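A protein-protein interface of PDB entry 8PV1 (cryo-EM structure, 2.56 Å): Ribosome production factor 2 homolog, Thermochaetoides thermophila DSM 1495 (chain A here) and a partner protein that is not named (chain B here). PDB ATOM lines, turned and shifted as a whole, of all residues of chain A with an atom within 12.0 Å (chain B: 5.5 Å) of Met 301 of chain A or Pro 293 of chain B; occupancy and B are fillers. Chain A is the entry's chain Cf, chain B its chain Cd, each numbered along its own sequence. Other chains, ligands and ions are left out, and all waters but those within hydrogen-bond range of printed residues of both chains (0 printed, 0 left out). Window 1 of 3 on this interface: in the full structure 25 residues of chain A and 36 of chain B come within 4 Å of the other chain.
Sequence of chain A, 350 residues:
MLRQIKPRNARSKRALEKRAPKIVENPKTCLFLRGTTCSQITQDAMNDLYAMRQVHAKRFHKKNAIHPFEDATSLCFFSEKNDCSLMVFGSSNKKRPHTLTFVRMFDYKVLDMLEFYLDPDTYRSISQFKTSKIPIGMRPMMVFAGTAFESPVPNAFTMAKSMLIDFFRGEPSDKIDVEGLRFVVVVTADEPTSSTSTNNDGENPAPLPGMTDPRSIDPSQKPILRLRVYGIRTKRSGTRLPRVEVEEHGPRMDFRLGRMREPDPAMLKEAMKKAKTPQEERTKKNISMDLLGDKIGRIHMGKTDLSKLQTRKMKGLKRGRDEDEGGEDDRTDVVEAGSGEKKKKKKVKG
The backbone NH of Ile 299 of chain A lies within hydrogen-bond range of the backbone carbonyl oxygen of Tyr 103 of chain B. N of His 300 of chain A sits at hydrogen-bond distance from OE1 of Gln 316 of chain B (2.9 Å).
The backbone carbonyl oxygen (O) of Pro 293 of chain B sits at hydrogen-bond distance from the backbone NH (N) of Phe 268 of chain B (2.9 Å). The backbone NH (N) of Cys 295 of chain B sits at hydrogen-bond distance from the backbone carbonyl oxygen (O) of Phe 268 of chain B (2.9 Å). O of His 292 of chain B sits at hydrogen-bond distance from OG1 of Thr 294 of chain B, 3.0 Å away. The backbone carbonyl oxygen (O) of Asn 286 of chain A is in hydrogen-bond range of the backbone NH (N) of Arg 298 of chain A (3.2 Å). OD1 of Asn 286 of chain A sits at hydrogen-bond distance from NE2 of His 300 of chain A (3.0 Å).
Among the printed residues, merely in contact across the chains: Met 301 of chain A with Thr 294 of chain B (3.4 Å), Ile 299 of chain A with Gln 316 of chain B (3.5 Å), Met 301 of chain A with Cys 295 of chain B (3.6 Å), Arg 298 of chain A with Tyr 103 of chain B (3.7 Å), Met 301 of chain A with Pro 293 of chain B (3.7 Å), Met 301 of chain A with Tyr 103 of chain B (3.7 Å), Ile 299 of chain A with Pro 293 of chain B (3.7 Å), Met 301 of chain A with Leu 313 of chain B (3.8 Å) and Ile 299 of chain A with Leu 313 of chain B (3.9 Å).
Met 301 of chain A touches five residues of chain B. Of the printed residues of chain A, Pro 293 of chain B touches Ile 299 and Met 301. No residue of chain A comes within 4 Å of Val 267 of chain B. No residue of chain A comes within 4 Å of Phe 268 of chain B. No residue of chain A comes within 4 Å of His 292 of chain B. No residue of chain A comes within 4 Å of Ser 309 of chain B. Of chain A, only Ile 299 and Met 301 come within 4 Å of Leu 313 of chain B. Printed residues of chain B within 4 Å of His 300 of chain A: Gln 316. Printed residues of chain A within 4 Å of Gln 316 of chain B: Ile 299 (3.5 Å) and His 300 (2.9 Å). The nearest printed residue of chain A that does not touch Gln 316 of chain B is Arg 298 of chain A (4.4 Å).
Of the 16 printed residues of chain B, 6 touch a printed residue of chain A. Of the 12 printed residues of chain A, 4 touch a printed residue of chain B. Hydrophobic or aromatic side chains of chain A within 4 Å of the printed part of chain B: Ile 299, His 300 and Met 301. Along chain A the printed residues that touch a printed residue of chain B span positions 298 to 301. Among the printed residues, no Asp or Glu carboxylate lies within 4 Å of a Lys or Arg side-chain nitrogen of the other chain.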
ATOM      1  N   ASN A 286       7.957  14.139   2.674  1.00  0.00           N
ATOM      2  CA  ASN A 286       6.821  13.283   2.334  1.00  0.00           C
ATOM      3  C   ASN A 286       5.473  13.976   2.500  1.00  0.00           C
ATOM      4  O   ASN A 286       4.443  13.298   2.580  1.00  0.00           O
ATOM      5  CB  ASN A 286       6.835  11.973   3.134  1.00  0.00           C
ATOM      6  CG  ASN A 286       8.070  11.144   2.867  1.00  0.00           C
ATOM      7  OD1 ASN A 286       8.546  11.069   1.736  1.00  0.00           O
ATOM      8  ND2 ASN A 286       8.602  10.522   3.909  1.00  0.00           N
ATOM      9  N   ILE A 296      -1.222  15.682   0.964  1.00  0.00           N
ATOM     10  CA  ILE A 296      -0.976  14.300   0.581  1.00  0.00           C
ATOM     11  C   ILE A 296       0.312  13.832   1.237  1.00  0.00           C
ATOM     12  O   ILE A 296       1.339  14.518   1.179  1.00  0.00           O
ATOM     13  CB  ILE A 296      -0.895  14.153  -0.954  1.00  0.00           C
ATOM     14  CG1 ILE A 296      -2.160  14.705  -1.611  1.00  0.00           C
ATOM     15  CG2 ILE A 296      -0.691  12.708  -1.345  1.00  0.00           C
ATOM     16  CD1 ILE A 296      -3.427  14.007  -1.184  1.00  0.00           C
ATOM     17  N   GLY A 297       0.252  12.665   1.871  1.00  0.00           N
ATOM     18  CA  GLY A 297       1.416  12.036   2.464  1.00  0.00           C
ATOM     19  C   GLY A 297       1.839  10.834   1.643  1.00  0.00           C
ATOM     20  O   GLY A 297       1.011  10.177   1.012  1.00  0.00           O
ATOM     21  N   ARG A 298       3.137  10.554   1.646  1.00  0.00           N
ATOM     22  CA  ARG A 298       3.700   9.445   0.891  1.00  0.00           C
ATOM     23  C   ARG A 298       4.290   8.420   1.847  1.00  0.00           C
ATOM     24  O   ARG A 298       5.060   8.772   2.745  1.00  0.00           O
ATOM     25  CB  ARG A 298       4.772   9.932  -0.084  1.00  0.00           C
ATOM     26  CG  ARG A 298       5.144   8.907  -1.138  1.00  0.00           C
ATOM     27  CD  ARG A 298       5.989   9.525  -2.247  1.00  0.00           C
ATOM     28  NE  ARG A 298       5.193  10.197  -3.271  1.00  0.00           N
ATOM     29  CZ  ARG A 298       4.395   9.595  -4.145  1.00  0.00           C
ATOM     30  NH1 ARG A 298       4.292   8.276  -4.202  1.00  0.00           N
ATOM     31  NH2 ARG A 298       3.692  10.335  -4.997  1.00  0.00           N
ATOM     32  N   ILE A 299       3.924   7.158   1.653  1.00  0.00           N
ATOM     33  CA  ILE A 299       4.476   6.053   2.424  1.00  0.00           C
ATOM     34  C   ILE A 299       5.364   5.231   1.504  1.00  0.00           C
ATOM     35  O   ILE A 299       5.172   5.202   0.283  1.00  0.00           O
ATOM     36  CB  ILE A 299       3.376   5.178   3.059  1.00  0.00           C
ATOM     37  CG1 ILE A 299       2.378   4.723   1.996  1.00  0.00           C
ATOM     38  CG2 ILE A 299       2.673   5.939   4.173  1.00  0.00           C
ATOM     39  CD1 ILE A 299       1.352   3.748   2.506  1.00  0.00           C
ATOM     40  N   HIS A 300       6.348   4.564   2.095  1.00  0.00           N
ATOM     41  CA  HIS A 300       7.356   3.827   1.341  1.00  0.00           C
ATOM     42  C   HIS A 300       7.405   2.400   1.863  1.00  0.00           C
ATOM     43  O   HIS A 300       7.900   2.152   2.968  1.00  0.00           O
ATOM     44  CB  HIS A 300       8.708   4.524   1.443  1.00  0.00           C
ATOM     45  CG  HIS A 300       8.653   5.970   1.064  1.00  0.00           C
ATOM     46  ND1 HIS A 300       8.686   6.398  -0.244  1.00  0.00           N
ATOM     47  CD2 HIS A 300       8.537   7.085   1.822  1.00  0.00           C
ATOM     48  CE1 HIS A 300       8.600   7.715  -0.276  1.00  0.00           C
ATOM     49  NE2 HIS A 300       8.515   8.157   0.965  1.00  0.00           N
ATOM     50  N   MET A 301       6.887   1.468   1.063  1.00  0.00           N
ATOM     51  CA  MET A 301       6.700   0.097   1.521  1.00  0.00           C
ATOM     52  C   MET A 301       8.022  -0.656   1.588  1.00  0.00           C
ATOM     53  O   MET A 301       8.269  -1.417   2.530  1.00  0.00           O
ATOM     54  CB  MET A 301       5.720  -0.622   0.597  1.00  0.00           C
ATOM     55  CG  MET A 301       4.317  -0.054   0.640  1.00  0.00           C
ATOM     56  SD  MET A 301       3.589  -0.174   2.278  1.00  0.00           S
ATOM     57  CE  MET A 301       3.375  -1.943   2.389  1.00  0.00           C
ATOM     58  N   GLY A 302       8.881  -0.461   0.598  1.00  0.00           N
ATOM     59  CA  GLY A 302      10.104  -1.224   0.493  1.00  0.00           C
ATOM     60  C   GLY A 302       9.904  -2.513  -0.289  1.00  0.00           C
ATOM     61  O   GLY A 302       8.784  -2.938  -0.579  1.00  0.00           O
ATOM     62  N   LYS A 303      11.023  -3.141  -0.640  1.00  0.00           N
ATOM     63  CA  LYS A 303      10.974  -4.370  -1.417  1.00  0.00           C
ATOM     64  C   LYS A 303      10.537  -5.542  -0.545  1.00  0.00           C
ATOM     65  O   LYS A 303      10.957  -5.672   0.607  1.00  0.00           O
ATOM     66  CB  LYS A 303      12.339  -4.660  -2.039  1.00  0.00           C
ATOM     67  N   THR A 304       9.684  -6.395  -1.105  1.00  0.00           N
ATOM     68  CA  THR A 304       9.223  -7.587  -0.404  1.00  0.00           C
ATOM     69  C   THR A 304      10.218  -8.719  -0.633  1.00  0.00           C
ATOM     70  O   THR A 304      10.382  -9.190  -1.762  1.00  0.00           O
ATOM     71  CB  THR A 304       7.832  -7.988  -0.885  1.00  0.00           C
ATOM     72  N   ASP A 305      10.877  -9.155   0.439  1.00  0.00           N
ATOM     73  CA  ASP A 305      11.903 -10.196   0.369  1.00  0.00           C
ATOM     74  C   ASP A 305      11.411 -11.404   1.157  1.00  0.00           C
ATOM     75  O   ASP A 305      11.645 -11.504   2.366  1.00  0.00           O
ATOM     76  CB  ASP A 305      13.238  -9.689   0.907  1.00  0.00           C
ATOM     77  N   LEU A 306      10.737 -12.321   0.470  1.00  0.00           N
ATOM     78  CA  LEU A 306      10.215 -13.533   1.082  1.00  0.00           C
ATOM     79  C   LEU A 306      11.185 -14.703   0.996  1.00  0.00           C
ATOM     80  O   LEU A 306      10.791 -15.840   1.271  1.00  0.00           O
ATOM     81  CB  LEU A 306       8.882 -13.921   0.438  1.00  0.00           C
ATOM     82  CG  LEU A 306       7.576 -13.491   1.114  1.00  0.00           C
ATOM     83  CD1 LEU A 306       7.564 -12.009   1.449  1.00  0.00           C
ATOM     84  CD2 LEU A 306       6.391 -13.849   0.236  1.00  0.00           C
ATOM     85  N   PRO B 102      -1.736   4.049  -4.914  1.00  0.00           N
ATOM     86  CA  PRO B 102      -1.874   3.335  -3.631  1.00  0.00           C
ATOM     87  C   PRO B 102      -0.886   3.770  -2.560  1.00  0.00           C
ATOM     88  O   PRO B 102      -1.157   3.555  -1.374  1.00  0.00           O
ATOM     89  CB  PRO B 102      -1.651   1.867  -4.022  1.00  0.00           C
ATOM     90  CG  PRO B 102      -1.923   1.812  -5.484  1.00  0.00           C
ATOM     91  CD  PRO B 102      -1.467   3.126  -6.027  1.00  0.00           C
ATOM     92  N   TYR B 103       0.238   4.373  -2.930  1.00  0.00           N
ATOM     93  CA  TYR B 103       1.275   4.727  -1.972  1.00  0.00           C
ATOM     94  C   TYR B 103       1.163   6.164  -1.483  1.00  0.00           C
ATOM     95  O   TYR B 103       2.067   6.645  -0.794  1.00  0.00           O
ATOM     96  CB  TYR B 103       2.653   4.477  -2.581  1.00  0.00           C
ATOM     97  CG  TYR B 103       2.821   3.059  -3.070  1.00  0.00           C
ATOM     98  CD1 TYR B 103       2.595   1.984  -2.219  1.00  0.00           C
ATOM     99  CD2 TYR B 103       3.191   2.793  -4.380  1.00  0.00           C
ATOM    100  CE1 TYR B 103       2.741   0.683  -2.658  1.00  0.00           C
ATOM    101  CE2 TYR B 103       3.340   1.495  -4.829  1.00  0.00           C
ATOM    102  CZ  TYR B 103       3.113   0.446  -3.964  1.00  0.00           C
ATOM    103  OH  TYR B 103       3.261  -0.847  -4.407  1.00  0.00           O
ATOM    104  N   LEU B 266      -6.209   2.619   4.745  1.00  0.00           N
ATOM    105  CA  LEU B 266      -6.481   1.188   4.715  1.00  0.00           C
ATOM    106  C   LEU B 266      -5.244   0.448   4.220  1.00  0.00           C
ATOM    107  O   LEU B 266      -4.746   0.731   3.126  1.00  0.00           O
ATOM    108  CB  LEU B 266      -7.681   0.887   3.819  1.00  0.00           C
ATOM    109  CG  LEU B 266      -8.076  -0.580   3.660  1.00  0.00           C
ATOM    110  CD1 LEU B 266      -8.427  -1.186   5.006  1.00  0.00           C
ATOM    111  CD2 LEU B 266      -9.235  -0.709   2.694  1.00  0.00           C
ATOM    112  N   VAL B 267      -4.755  -0.496   5.021  1.00  0.00           N
ATOM    113  CA  VAL B 267      -3.569  -1.277   4.693  1.00  0.00           C
ATOM    114  C   VAL B 267      -3.912  -2.758   4.786  1.00  0.00           C
ATOM    115  O   VAL B 267      -4.425  -3.222   5.810  1.00  0.00           O
ATOM    116  CB  VAL B 267      -2.390  -0.925   5.626  1.00  0.00           C
ATOM    117  CG1 VAL B 267      -1.246  -1.910   5.457  1.00  0.00           C
ATOM    118  CG2 VAL B 267      -1.912   0.495   5.367  1.00  0.00           C
ATOM    119  N   PHE B 268      -3.632  -3.497   3.714  1.00  0.00           N
ATOM    120  CA  PHE B 268      -3.815  -4.941   3.696  1.00  0.00           C
ATOM    121  C   PHE B 268      -2.667  -5.622   4.425  1.00  0.00           C
ATOM    122  O   PHE B 268      -1.498  -5.289   4.216  1.00  0.00           O
ATOM    123  CB  PHE B 268      -3.879  -5.471   2.264  1.00  0.00           C
ATOM    124  CG  PHE B 268      -5.183  -5.214   1.574  1.00  0.00           C
ATOM    125  CD1 PHE B 268      -6.379  -5.322   2.257  1.00  0.00           C
ATOM    126  CD2 PHE B 268      -5.210  -4.893   0.229  1.00  0.00           C
ATOM    127  CE1 PHE B 268      -7.579  -5.092   1.617  1.00  0.00           C
ATOM    128  CE2 PHE B 268      -6.407  -4.665  -0.417  1.00  0.00           C
ATOM    129  CZ  PHE B 268      -7.591  -4.764   0.278  1.00  0.00           C
ATOM    130  N   VAL B 269      -3.002  -6.582   5.279  1.00  0.00           N
ATOM    131  CA  VAL B 269      -2.010  -7.442   5.912  1.00  0.00           C
ATOM    132  C   VAL B 269      -2.360  -8.875   5.547  1.00  0.00           C
ATOM    133  O   VAL B 269      -3.383  -9.403   5.998  1.00  0.00           O
ATOM    134  CB  VAL B 269      -1.956  -7.266   7.435  1.00  0.00           C
ATOM    135  CG1 VAL B 269      -0.838  -8.115   8.011  1.00  0.00           C
ATOM    136  CG2 VAL B 269      -1.760  -5.805   7.806  1.00  0.00           C
ATOM    137  N   LEU B 288      -2.771  -7.475  -4.716  1.00  0.00           N
ATOM    138  CA  LEU B 288      -3.403  -6.605  -3.725  1.00  0.00           C
ATOM    139  C   LEU B 288      -2.789  -5.207  -3.695  1.00  0.00           C
ATOM    140  O   LEU B 288      -3.477  -4.237  -3.343  1.00  0.00           O
ATOM    141  CB  LEU B 288      -3.323  -7.244  -2.342  1.00  0.00           C
ATOM    142  CG  LEU B 288      -4.210  -8.469  -2.128  1.00  0.00           C
ATOM    143  CD1 LEU B 288      -3.763  -9.252  -0.908  1.00  0.00           C
ATOM    144  CD2 LEU B 288      -5.664  -8.053  -2.000  1.00  0.00           C
ATOM    145  N   GLN B 289      -1.509  -5.077  -4.050  1.00  0.00           N
ATOM    146  CA  GLN B 289      -0.852  -3.776  -3.996  1.00  0.00           C
ATOM    147  C   GLN B 289      -1.295  -2.844  -5.114  1.00  0.00           C
ATOM    148  O   GLN B 289      -0.963  -1.655  -5.068  1.00  0.00           O
ATOM    149  CB  GLN B 289       0.666  -3.944  -4.030  1.00  0.00           C
ATOM    150  CG  GLN B 289       1.222  -4.344  -5.380  1.00  0.00           C
ATOM    151  CD  GLN B 289       2.681  -4.732  -5.308  1.00  0.00           C
ATOM    152  OE1 GLN B 289       3.258  -4.818  -4.224  1.00  0.00           O
ATOM    153  NE2 GLN B 289       3.289  -4.971  -6.463  1.00  0.00           N
ATOM    154  N   ASP B 291      -4.379  -2.150  -5.415  1.00  0.00           N
ATOM    155  CA  ASP B 291      -5.440  -1.444  -4.709  1.00  0.00           C
ATOM    156  C   ASP B 291      -4.950  -0.758  -3.441  1.00  0.00           C
ATOM    157  O   ASP B 291      -5.168   0.443  -3.266  1.00  0.00           O
ATOM    158  CB  ASP B 291      -6.579  -2.411  -4.363  1.00  0.00           C
ATOM    159  CG  ASP B 291      -7.292  -2.930  -5.590  1.00  0.00           C
ATOM    160  OD1 ASP B 291      -7.064  -2.381  -6.688  1.00  0.00           O
ATOM    161  OD2 ASP B 291      -8.081  -3.887  -5.459  1.00  0.00           O
ATOM    162  N   HIS B 292      -4.294  -1.492  -2.547  1.00  0.00           N
ATOM    163  CA  HIS B 292      -3.920  -0.939  -1.254  1.00  0.00           C
ATOM    164  C   HIS B 292      -2.557  -1.471  -0.843  1.00  0.00           C
ATOM    165  O   HIS B 292      -2.165  -2.560  -1.273  1.00  0.00           O
ATOM    166  CB  HIS B 292      -4.974  -1.281  -0.188  1.00  0.00           C
ATOM    167  CG  HIS B 292      -6.267  -0.548  -0.368  1.00  0.00           C
ATOM    168  ND1 HIS B 292      -7.357  -1.104  -1.000  1.00  0.00           N
ATOM    169  CD2 HIS B 292      -6.634   0.708  -0.018  1.00  0.00           C
ATOM    170  CE1 HIS B 292      -8.346  -0.229  -1.019  1.00  0.00           C
ATOM    171  NE2 HIS B 292      -7.933   0.879  -0.431  1.00  0.00           N
ATOM    172  N   PRO B 293      -1.804  -0.719  -0.034  1.00  0.00           N
ATOM    173  CA  PRO B 293      -0.490  -1.202   0.416  1.00  0.00           C
ATOM    174  C   PRO B 293      -0.613  -2.470   1.248  1.00  0.00           C
ATOM    175  O   PRO B 293      -1.392  -2.535   2.197  1.00  0.00           O
ATOM    176  CB  PRO B 293       0.048  -0.037   1.252  1.00  0.00           C
ATOM    177  CG  PRO B 293      -0.713   1.143   0.816  1.00  0.00           C
ATOM    178  CD  PRO B 293      -2.060   0.663   0.411  1.00  0.00           C
ATOM    179  N   THR B 294       0.180  -3.478   0.892  1.00  0.00           N
ATOM    180  CA  THR B 294       0.054  -4.811   1.462  1.00  0.00           C
ATOM    181  C   THR B 294       1.352  -5.227   2.137  1.00  0.00           C
ATOM    182  O   THR B 294       2.437  -5.071   1.571  1.00  0.00           O
ATOM    183  CB  THR B 294      -0.323  -5.835   0.384  1.00  0.00           C
ATOM    184  OG1 THR B 294      -1.423  -5.335  -0.381  1.00  0.00           O
ATOM    185  CG2 THR B 294      -0.722  -7.161   1.010  1.00  0.00           C
ATOM    186  N   CYS B 295       1.229  -5.751   3.353  1.00  0.00           N
ATOM    187  CA  CYS B 295       2.342  -6.317   4.099  1.00  0.00           C
ATOM    188  C   CYS B 295       2.097  -7.801   4.328  1.00  0.00           C
ATOM    189  O   CYS B 295       1.032  -8.190   4.809  1.00  0.00           O
ATOM    190  CB  CYS B 295       2.522  -5.625   5.455  1.00  0.00           C
ATOM    191  SG  CYS B 295       2.756  -3.843   5.395  1.00  0.00           S
ATOM    192  N   SER B 309       8.837  -4.587   8.859  1.00  0.00           N
ATOM    193  CA  SER B 309       8.190  -3.821   7.799  1.00  0.00           C
ATOM    194  C   SER B 309       6.891  -3.185   8.282  1.00  0.00           C
ATOM    195  O   SER B 309       6.612  -2.014   7.990  1.00  0.00           O
ATOM    196  CB  SER B 309       7.929  -4.722   6.592  1.00  0.00           C
ATOM    197  OG  SER B 309       9.144  -5.194   6.038  1.00  0.00           O
ATOM    198  N   LEU B 313       6.102   0.820   8.635  1.00  0.00           N
ATOM    199  CA  LEU B 313       4.972   1.491   7.995  1.00  0.00           C
ATOM    200  C   LEU B 313       4.133   2.263   9.011  1.00  0.00           C
ATOM    201  O   LEU B 313       3.698   3.396   8.748  1.00  0.00           O
ATOM    202  CB  LEU B 313       4.116   0.467   7.249  1.00  0.00           C
ATOM    203  CG  LEU B 313       2.875   0.989   6.524  1.00  0.00           C
ATOM    204  CD1 LEU B 313       3.237   2.113   5.566  1.00  0.00           C
ATOM    205  CD2 LEU B 313       2.182  -0.140   5.789  1.00  0.00           C
ATOM    206  N   GLN B 316       5.963   5.398   9.848  1.00  0.00           N
ATOM    207  CA  GLN B 316       5.778   6.408   8.810  1.00  0.00           C
ATOM    208  C   GLN B 316       4.427   7.098   8.946  1.00  0.00           C
ATOM    209  O   GLN B 316       4.328   8.318   8.771  1.00  0.00           O
ATOM    210  CB  GLN B 316       5.921   5.781   7.425  1.00  0.00           C
ATOM    211  CG  GLN B 316       7.293   5.217   7.133  1.00  0.00           C
ATOM    212  CD  GLN B 316       7.415   4.712   5.716  1.00  0.00           C
ATOM    213  OE1 GLN B 316       6.926   5.340   4.780  1.00  0.00           O
ATOM    214  NE2 GLN B 316       8.061   3.568   5.549  1.00  0.00           N
